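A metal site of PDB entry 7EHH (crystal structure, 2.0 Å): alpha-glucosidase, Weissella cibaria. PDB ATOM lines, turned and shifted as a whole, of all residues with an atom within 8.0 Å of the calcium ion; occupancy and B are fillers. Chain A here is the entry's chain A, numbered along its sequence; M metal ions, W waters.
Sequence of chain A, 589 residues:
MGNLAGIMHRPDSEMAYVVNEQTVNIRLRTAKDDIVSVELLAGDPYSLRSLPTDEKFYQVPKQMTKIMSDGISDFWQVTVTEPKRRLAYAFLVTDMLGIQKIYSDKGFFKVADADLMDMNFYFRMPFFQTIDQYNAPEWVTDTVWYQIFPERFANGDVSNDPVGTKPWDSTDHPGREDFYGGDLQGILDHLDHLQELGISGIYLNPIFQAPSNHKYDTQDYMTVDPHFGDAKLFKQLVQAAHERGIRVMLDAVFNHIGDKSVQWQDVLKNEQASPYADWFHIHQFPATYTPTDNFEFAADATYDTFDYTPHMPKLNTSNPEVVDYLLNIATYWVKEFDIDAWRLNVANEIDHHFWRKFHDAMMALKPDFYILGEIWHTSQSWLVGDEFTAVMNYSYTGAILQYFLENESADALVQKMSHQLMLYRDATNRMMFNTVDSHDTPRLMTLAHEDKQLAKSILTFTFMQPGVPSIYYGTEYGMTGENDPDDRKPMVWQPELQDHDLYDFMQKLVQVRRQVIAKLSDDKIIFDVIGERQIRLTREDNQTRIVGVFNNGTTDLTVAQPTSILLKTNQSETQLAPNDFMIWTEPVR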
ATOM      1  N   PRO A 150       3.750 -13.458  36.141  1.00  0.00           N
ATOM      2  CA  PRO A 150       2.641 -14.162  35.469  1.00  0.00           C
ATOM      3  C   PRO A 150       2.889 -14.507  34.003  1.00  0.00           C
ATOM      4  O   PRO A 150       2.368 -15.523  33.526  1.00  0.00           O
ATOM      5  CB  PRO A 150       1.466 -13.186  35.606  1.00  0.00           C
ATOM      6  CG  PRO A 150       1.822 -12.317  36.770  1.00  0.00           C
ATOM      7  CD  PRO A 150       3.318 -12.168  36.717  1.00  0.00           C
ATOM      8  N   GLU A 151       3.663 -13.698  33.281  1.00  0.00           N
ATOM      9  CA  GLU A 151       3.919 -14.002  31.875  1.00  0.00           C
ATOM     10  C   GLU A 151       4.707 -15.286  31.690  1.00  0.00           C
ATOM     11  O   GLU A 151       4.736 -15.822  30.570  1.00  0.00           O
ATOM     12  CB  GLU A 151       4.665 -12.839  31.215  1.00  0.00           C
ATOM     13  CG  GLU A 151       4.145 -12.414  29.843  1.00  0.00           C
ATOM     14  CD  GLU A 151       4.501 -13.378  28.721  1.00  0.00           C
ATOM     15  OE1 GLU A 151       3.595 -13.744  27.945  1.00  0.00           O
ATOM     16  OE2 GLU A 151       5.689 -13.763  28.619  1.00  0.00           O
ATOM     17  N   ALA A 154       2.667 -20.107  33.717  1.00  0.00           N
ATOM     18  CA  ALA A 154       1.950 -21.157  33.005  1.00  0.00           C
ATOM     19  C   ALA A 154       0.978 -20.534  32.015  1.00  0.00           C
ATOM     20  O   ALA A 154       0.244 -19.602  32.364  1.00  0.00           O
ATOM     21  CB  ALA A 154       1.204 -22.082  33.985  1.00  0.00           C
ATOM     22  N   ASN A 155       0.963 -21.075  30.801  1.00  0.00           N
ATOM     23  CA  ASN A 155       0.031 -20.640  29.764  1.00  0.00           C
ATOM     24  C   ASN A 155      -1.194 -21.550  29.828  1.00  0.00           C
ATOM     25  O   ASN A 155      -1.171 -22.668  29.307  1.00  0.00           O
ATOM     26  CB  ASN A 155       0.709 -20.680  28.395  1.00  0.00           C
ATOM     27  CG  ASN A 155      -0.181 -20.152  27.281  1.00  0.00           C
ATOM     28  OD1 ASN A 155      -1.286 -19.655  27.523  1.00  0.00           O
ATOM     29  ND2 ASN A 155       0.300 -20.241  26.044  1.00  0.00           N
ATOM     30  N   GLY A 156      -2.247 -21.078  30.470  1.00  0.00           N
ATOM     31  CA  GLY A 156      -3.498 -21.811  30.557  1.00  0.00           C
ATOM     32  C   GLY A 156      -4.494 -21.481  29.463  1.00  0.00           C
ATOM     33  O   GLY A 156      -5.619 -21.992  29.507  1.00  0.00           O
ATOM     34  N   ASP A 157      -4.110 -20.644  28.504  1.00  0.00           N
ATOM     35  CA  ASP A 157      -5.031 -20.188  27.467  1.00  0.00           C
ATOM     36  C   ASP A 157      -4.270 -19.628  26.281  1.00  0.00           C
ATOM     37  O   ASP A 157      -3.822 -18.475  26.316  1.00  0.00           O
ATOM     38  CB  ASP A 157      -5.980 -19.128  28.033  1.00  0.00           C
ATOM     39  CG  ASP A 157      -7.104 -18.764  27.082  1.00  0.00           C
ATOM     40  OD1 ASP A 157      -7.098 -19.224  25.929  1.00  0.00           O
ATOM     41  OD2 ASP A 157      -8.003 -17.997  27.502  1.00  0.00           O
ATOM     42  N   VAL A 158      -4.096 -20.415  25.217  1.00  0.00           N
ATOM     43  CA  VAL A 158      -3.380 -19.938  24.039  1.00  0.00           C
ATOM     44  C   VAL A 158      -4.152 -18.847  23.313  1.00  0.00           C
ATOM     45  O   VAL A 158      -3.566 -18.114  22.508  1.00  0.00           O
ATOM     46  CB  VAL A 158      -3.062 -21.089  23.071  1.00  0.00           C
ATOM     47  CG1 VAL A 158      -2.001 -22.007  23.653  1.00  0.00           C
ATOM     48  CG2 VAL A 158      -4.329 -21.868  22.730  1.00  0.00           C
ATOM     49  N   SER A 159      -5.461 -18.732  23.553  1.00  0.00           N
ATOM     50  CA  SER A 159      -6.352 -17.815  22.854  1.00  0.00           C
ATOM     51  C   SER A 159      -6.055 -16.348  23.157  1.00  0.00           C
ATOM     52  O   SER A 159      -6.513 -15.477  22.410  1.00  0.00           O
ATOM     53  CB  SER A 159      -7.811 -18.133  23.200  1.00  0.00           C
ATOM     54  OG  SER A 159      -8.175 -17.563  24.450  1.00  0.00           O
ATOM     55  N   ASN A 160      -5.454 -16.071  24.311  1.00  0.00           N
ATOM     56  CA  ASN A 160      -5.146 -14.705  24.711  1.00  0.00           C
ATOM     57  C   ASN A 160      -3.670 -14.376  24.557  1.00  0.00           C
ATOM     58  O   ASN A 160      -3.221 -13.342  25.078  1.00  0.00           O
ATOM     59  CB  ASN A 160      -5.618 -14.441  26.151  1.00  0.00           C
ATOM     60  CG  ASN A 160      -4.926 -15.339  27.171  1.00  0.00           C
ATOM     61  OD1 ASN A 160      -3.829 -15.860  26.942  1.00  0.00           O
ATOM     62  ND2 ASN A 160      -5.563 -15.504  28.330  1.00  0.00           N
ATOM     63  N   ASP A 161      -2.902 -15.216  23.872  1.00  0.00           N
ATOM     64  CA  ASP A 161      -1.477 -14.994  23.752  1.00  0.00           C
ATOM     65  C   ASP A 161      -1.204 -13.743  22.905  1.00  0.00           C
ATOM     66  O   ASP A 161      -1.895 -13.507  21.912  1.00  0.00           O
ATOM     67  CB  ASP A 161      -0.789 -16.201  23.110  1.00  0.00           C
ATOM     68  CG  ASP A 161      -0.706 -17.388  24.051  1.00  0.00           C
ATOM     69  OD1 ASP A 161      -1.083 -17.250  25.230  1.00  0.00           O
ATOM     70  OD2 ASP A 161      -0.262 -18.480  23.615  1.00  0.00           O
ATOM     71  N   PRO A 162      -0.209 -12.943  23.275  1.00  0.00           N
ATOM     72  CA  PRO A 162       0.173 -11.806  22.433  1.00  0.00           C
ATOM     73  C   PRO A 162       0.728 -12.282  21.093  1.00  0.00           C
ATOM     74  O   PRO A 162       1.081 -13.446  20.905  1.00  0.00           O
ATOM     75  CB  PRO A 162       1.268 -11.106  23.251  1.00  0.00           C
ATOM     76  CG  PRO A 162       1.062 -11.580  24.663  1.00  0.00           C
ATOM     77  CD  PRO A 162       0.547 -12.987  24.535  1.00  0.00           C
ATOM     78  N   THR A 165       3.988 -14.813  20.214  1.00  0.00           N
ATOM     79  CA  THR A 165       4.285 -15.617  21.430  1.00  0.00           C
ATOM     80  C   THR A 165       5.181 -16.793  21.026  1.00  0.00           C
ATOM     81  O   THR A 165       4.849 -17.456  20.038  1.00  0.00           O
ATOM     82  CB  THR A 165       2.985 -16.113  22.083  1.00  0.00           C
ATOM     83  OG1 THR A 165       2.337 -14.994  22.660  1.00  0.00           O
ATOM     84  CG2 THR A 165       3.232 -17.177  23.130  1.00  0.00           C
ATOM     85  N   TRP A 168       6.646 -22.528  24.553  1.00  0.00           N
ATOM     86  CA  TRP A 168       7.049 -22.626  25.972  1.00  0.00           C
ATOM     87  C   TRP A 168       8.336 -23.446  26.127  1.00  0.00           C
ATOM     88  O   TRP A 168       8.257 -24.668  25.982  1.00  0.00           O
ATOM     89  CB  TRP A 168       5.919 -23.194  26.827  1.00  0.00           C
ATOM     90  CG  TRP A 168       6.065 -22.881  28.276  1.00  0.00           C
ATOM     91  CD1 TRP A 168       6.809 -23.562  29.199  1.00  0.00           C
ATOM     92  CD2 TRP A 168       5.470 -21.767  28.979  1.00  0.00           C
ATOM     93  NE1 TRP A 168       6.702 -22.966  30.420  1.00  0.00           N
ATOM     94  CE2 TRP A 168       5.896 -21.861  30.315  1.00  0.00           C
ATOM     95  CE3 TRP A 168       4.637 -20.714  28.608  1.00  0.00           C
ATOM     96  CZ2 TRP A 168       5.492 -20.950  31.289  1.00  0.00           C
ATOM     97  CZ3 TRP A 168       4.246 -19.809  29.563  1.00  0.00           C
ATOM     98  CH2 TRP A 168       4.667 -19.919  30.884  1.00  0.00           C
ATOM     99  N   TYR A 180       5.689 -15.384  26.254  1.00  0.00           N
ATOM    100  CA  TYR A 180       5.517 -16.858  26.281  1.00  0.00           C
ATOM    101  C   TYR A 180       4.040 -17.215  26.490  1.00  0.00           C
ATOM    102  O   TYR A 180       3.692 -18.390  26.333  1.00  0.00           O
ATOM    103  CB  TYR A 180       6.487 -17.520  27.259  1.00  0.00           C
ATOM    104  CG  TYR A 180       7.921 -17.545  26.767  1.00  0.00           C
ATOM    105  CD1 TYR A 180       8.799 -16.526  27.072  1.00  0.00           C
ATOM    106  CD2 TYR A 180       8.383 -18.583  25.980  1.00  0.00           C
ATOM    107  CE1 TYR A 180      10.109 -16.544  26.632  1.00  0.00           C
ATOM    108  CE2 TYR A 180       9.689 -18.617  25.524  1.00  0.00           C
ATOM    109  CZ  TYR A 180      10.554 -17.592  25.847  1.00  0.00           C
ATOM    110  OH  TYR A 180      11.849 -17.603  25.410  1.00  0.00           O
ATOM    111  N   GLY A 181       3.211 -16.245  26.889  1.00  0.00           N
ATOM    112  CA  GLY A 181       1.784 -16.507  26.997  1.00  0.00           C
ATOM    113  C   GLY A 181       1.267 -16.885  28.367  1.00  0.00           C
ATOM    114  O   GLY A 181       0.130 -17.342  28.468  1.00  0.00           O
ATOM    115  N   GLY A 182       2.060 -16.707  29.426  1.00  0.00           N
ATOM    116  CA  GLY A 182       1.562 -17.003  30.756  1.00  0.00           C
ATOM    117  C   GLY A 182       0.410 -16.096  31.142  1.00  0.00           C
ATOM    118  O   GLY A 182       0.362 -14.924  30.785  1.00  0.00           O
ATOM    119  N   ASP A 183      -0.531 -16.653  31.913  1.00  0.00           N
ATOM    120  CA  ASP A 183      -1.768 -15.944  32.215  1.00  0.00           C
ATOM    121  C   ASP A 183      -2.320 -16.432  33.551  1.00  0.00           C
ATOM    122  O   ASP A 183      -1.722 -17.280  34.231  1.00  0.00           O
ATOM    123  CB  ASP A 183      -2.785 -16.128  31.080  1.00  0.00           C
ATOM    124  CG  ASP A 183      -2.922 -17.583  30.648  1.00  0.00           C
ATOM    125  OD1 ASP A 183      -3.063 -18.462  31.524  1.00  0.00           O
ATOM    126  OD2 ASP A 183      -2.910 -17.840  29.421  1.00  0.00           O
ATOM    127  N   LEU A 184      -3.484 -15.902  33.930  1.00  0.00           N
ATOM    128  CA  LEU A 184      -4.094 -16.255  35.210  1.00  0.00           C
ATOM    129  C   LEU A 184      -4.636 -17.673  35.194  1.00  0.00           C
ATOM    130  O   LEU A 184      -4.640 -18.343  36.246  1.00  0.00           O
ATOM    131  CB  LEU A 184      -5.213 -15.273  35.554  1.00  0.00           C
ATOM    132  CG  LEU A 184      -4.823 -13.800  35.704  1.00  0.00           C
ATOM    133  CD1 LEU A 184      -6.053 -12.972  36.039  1.00  0.00           C
ATOM    134  CD2 LEU A 184      -3.751 -13.629  36.763  1.00  0.00           C
ATOM    135  N   GLN A 185      -5.116 -18.146  34.042  1.00  0.00           N
ATOM    136  CA  GLN A 185      -5.631 -19.503  33.955  1.00  0.00           C
ATOM    137  C   GLN A 185      -4.554 -20.527  34.292  1.00  0.00           C
ATOM    138  O   GLN A 185      -4.863 -21.561  34.887  1.00  0.00           O
ATOM    139  CB  GLN A 185      -6.215 -19.759  32.568  1.00  0.00           C
ATOM    140  CG  GLN A 185      -6.917 -21.104  32.415  1.00  0.00           C
ATOM    141  CD  GLN A 185      -8.149 -21.230  33.304  1.00  0.00           C
ATOM    142  OE1 GLN A 185      -9.061 -20.401  33.248  1.00  0.00           O
ATOM    143  NE2 GLN A 185      -8.176 -22.265  34.129  1.00  0.00           N
ATOM    144  N   GLY A 186      -3.294 -20.248  33.934  1.00  0.00           N
ATOM    145  CA  GLY A 186      -2.223 -21.172  34.290  1.00  0.00           C
ATOM    146  C   GLY A 186      -1.979 -21.255  35.783  1.00  0.00           C
ATOM    147  O   GLY A 186      -1.735 -22.345  36.330  1.00  0.00           O
ATOM    148  N   PRO A 226      -5.724  -8.008  29.216  1.00  0.00           N
ATOM    149  CA  PRO A 226      -6.522  -8.933  28.400  1.00  0.00           C
ATOM    150  C   PRO A 226      -5.757 -10.228  28.081  1.00  0.00           C
ATOM    151  O   PRO A 226      -6.385 -11.250  27.925  1.00  0.00           O
ATOM    152  CB  PRO A 226      -6.889  -8.135  27.146  1.00  0.00           C
ATOM    153  CG  PRO A 226      -5.919  -6.985  27.115  1.00  0.00           C
ATOM    154  CD  PRO A 226      -5.571  -6.704  28.561  1.00  0.00           C
ATOM    155  N   HIS A 227      -4.434 -10.128  27.895  1.00  0.00           N
ATOM    156  CA  HIS A 227      -3.585 -11.319  27.687  1.00  0.00           C
ATOM    157  C   HIS A 227      -3.603 -12.213  28.936  1.00  0.00           C
ATOM    158  O   HIS A 227      -3.362 -13.394  28.781  1.00  0.00           O
ATOM    159  CB  HIS A 227      -2.191 -10.895  27.204  1.00  0.00           C
ATOM    160  CG  HIS A 227      -2.271 -10.048  25.975  1.00  0.00           C
ATOM    161  ND1 HIS A 227      -2.063  -8.688  26.010  1.00  0.00           N
ATOM    162  CD2 HIS A 227      -2.580 -10.360  24.707  1.00  0.00           C
ATOM    163  CE1 HIS A 227      -2.215  -8.207  24.800  1.00  0.00           C
ATOM    164  NE2 HIS A 227      -2.529  -9.201  23.977  1.00  0.00           N
ATOM    165  N   PHE A 228      -3.647 -11.611  30.131  1.00  0.00           N
ATOM    166  CA  PHE A 228      -3.718 -12.333  31.436  1.00  0.00           C
ATOM    167  C   PHE A 228      -5.106 -12.940  31.712  1.00  0.00           C
ATOM    168  O   PHE A 228      -5.172 -14.026  32.279  1.00  0.00           O
ATOM    169  CB  PHE A 228      -3.207 -11.460  32.573  1.00  0.00           C
ATOM    170  CG  PHE A 228      -1.714 -11.273  32.568  1.00  0.00           C
ATOM    171  CD1 PHE A 228      -0.925 -11.952  31.656  1.00  0.00           C
ATOM    172  CD2 PHE A 228      -1.094 -10.405  33.453  1.00  0.00           C
ATOM    173  CE1 PHE A 228       0.456 -11.773  31.642  1.00  0.00           C
ATOM    174  CE2 PHE A 228       0.270 -10.236  33.440  1.00  0.00           C
ATOM    175  CZ  PHE A 228       1.050 -10.920  32.530  1.00  0.00           C
ATOM    176  N   GLY A 229      -6.172 -12.205  31.386  1.00  0.00           N
ATOM    177  CA  GLY A 229      -7.553 -12.665  31.640  1.00  0.00           C
ATOM    178  C   GLY A 229      -8.508 -11.508  31.857  1.00  0.00           C
ATOM    179  O   GLY A 229      -8.295 -10.449  31.246  1.00  0.00           O
HETATM  180 CA    CA M   1      -1.996 -17.306  27.332  1.00  0.00          CA
HETATM  181  O   HOH W   1      -1.315 -14.960  27.496  1.00  0.00           O
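The side-chain carboxylate of Asp 183 is in hydrogen-bond range of the backbone NH of Gly 156, 2.9 Å away.
N of Asp 183 sits at hydrogen-bond distance from O of Ala 154 (3.1 Å).
The backbone NH (N) of Gln 185 lies within hydrogen-bond range of the side-chain carboxylate (OD1) of Asp 183.
The side-chain carboxylate (OD1) of Asp 183 sits at hydrogen-bond distance from the backbone NH (N) of Gly 186 (3.0 Å).
ND2 of Asn 160 lies close to O of His 227 (3.1 Å).
The side-chain carboxylate (OD1) of Asp 157 lies within hydrogen-bond range of the side-chain hydroxyl (OG) of Ser 159, at 2.5 Å.
N of Gly 181 is in hydrogen-bond range of OE1 of Glu 151 (2.7 Å).
Water W1 lies within hydrogen-bond range of O of His 227 (2.9 Å) and O of Asn 160 (3.5 Å).
Of the 24 residues printed, 6 come within 4 Å of the calcium ion.
OD1 of Asp 161 binds the calcium ion (2.3 Å).
The calcium ion is bound by OD2 of Asp 183.
OD1 of Asn 160 binds the calcium ion, at 2.4 Å.
The calcium ion is bound by O of Asp 157 (2.4 Å).
The backbone carbonyl oxygen (O) of Gly 181 binds the calcium ion (2.4 Å).
Water W1 binds the calcium ion.
The side-chain amide oxygen (OD1) of Asn 155 is bound to the calcium ion (2.5 Å).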
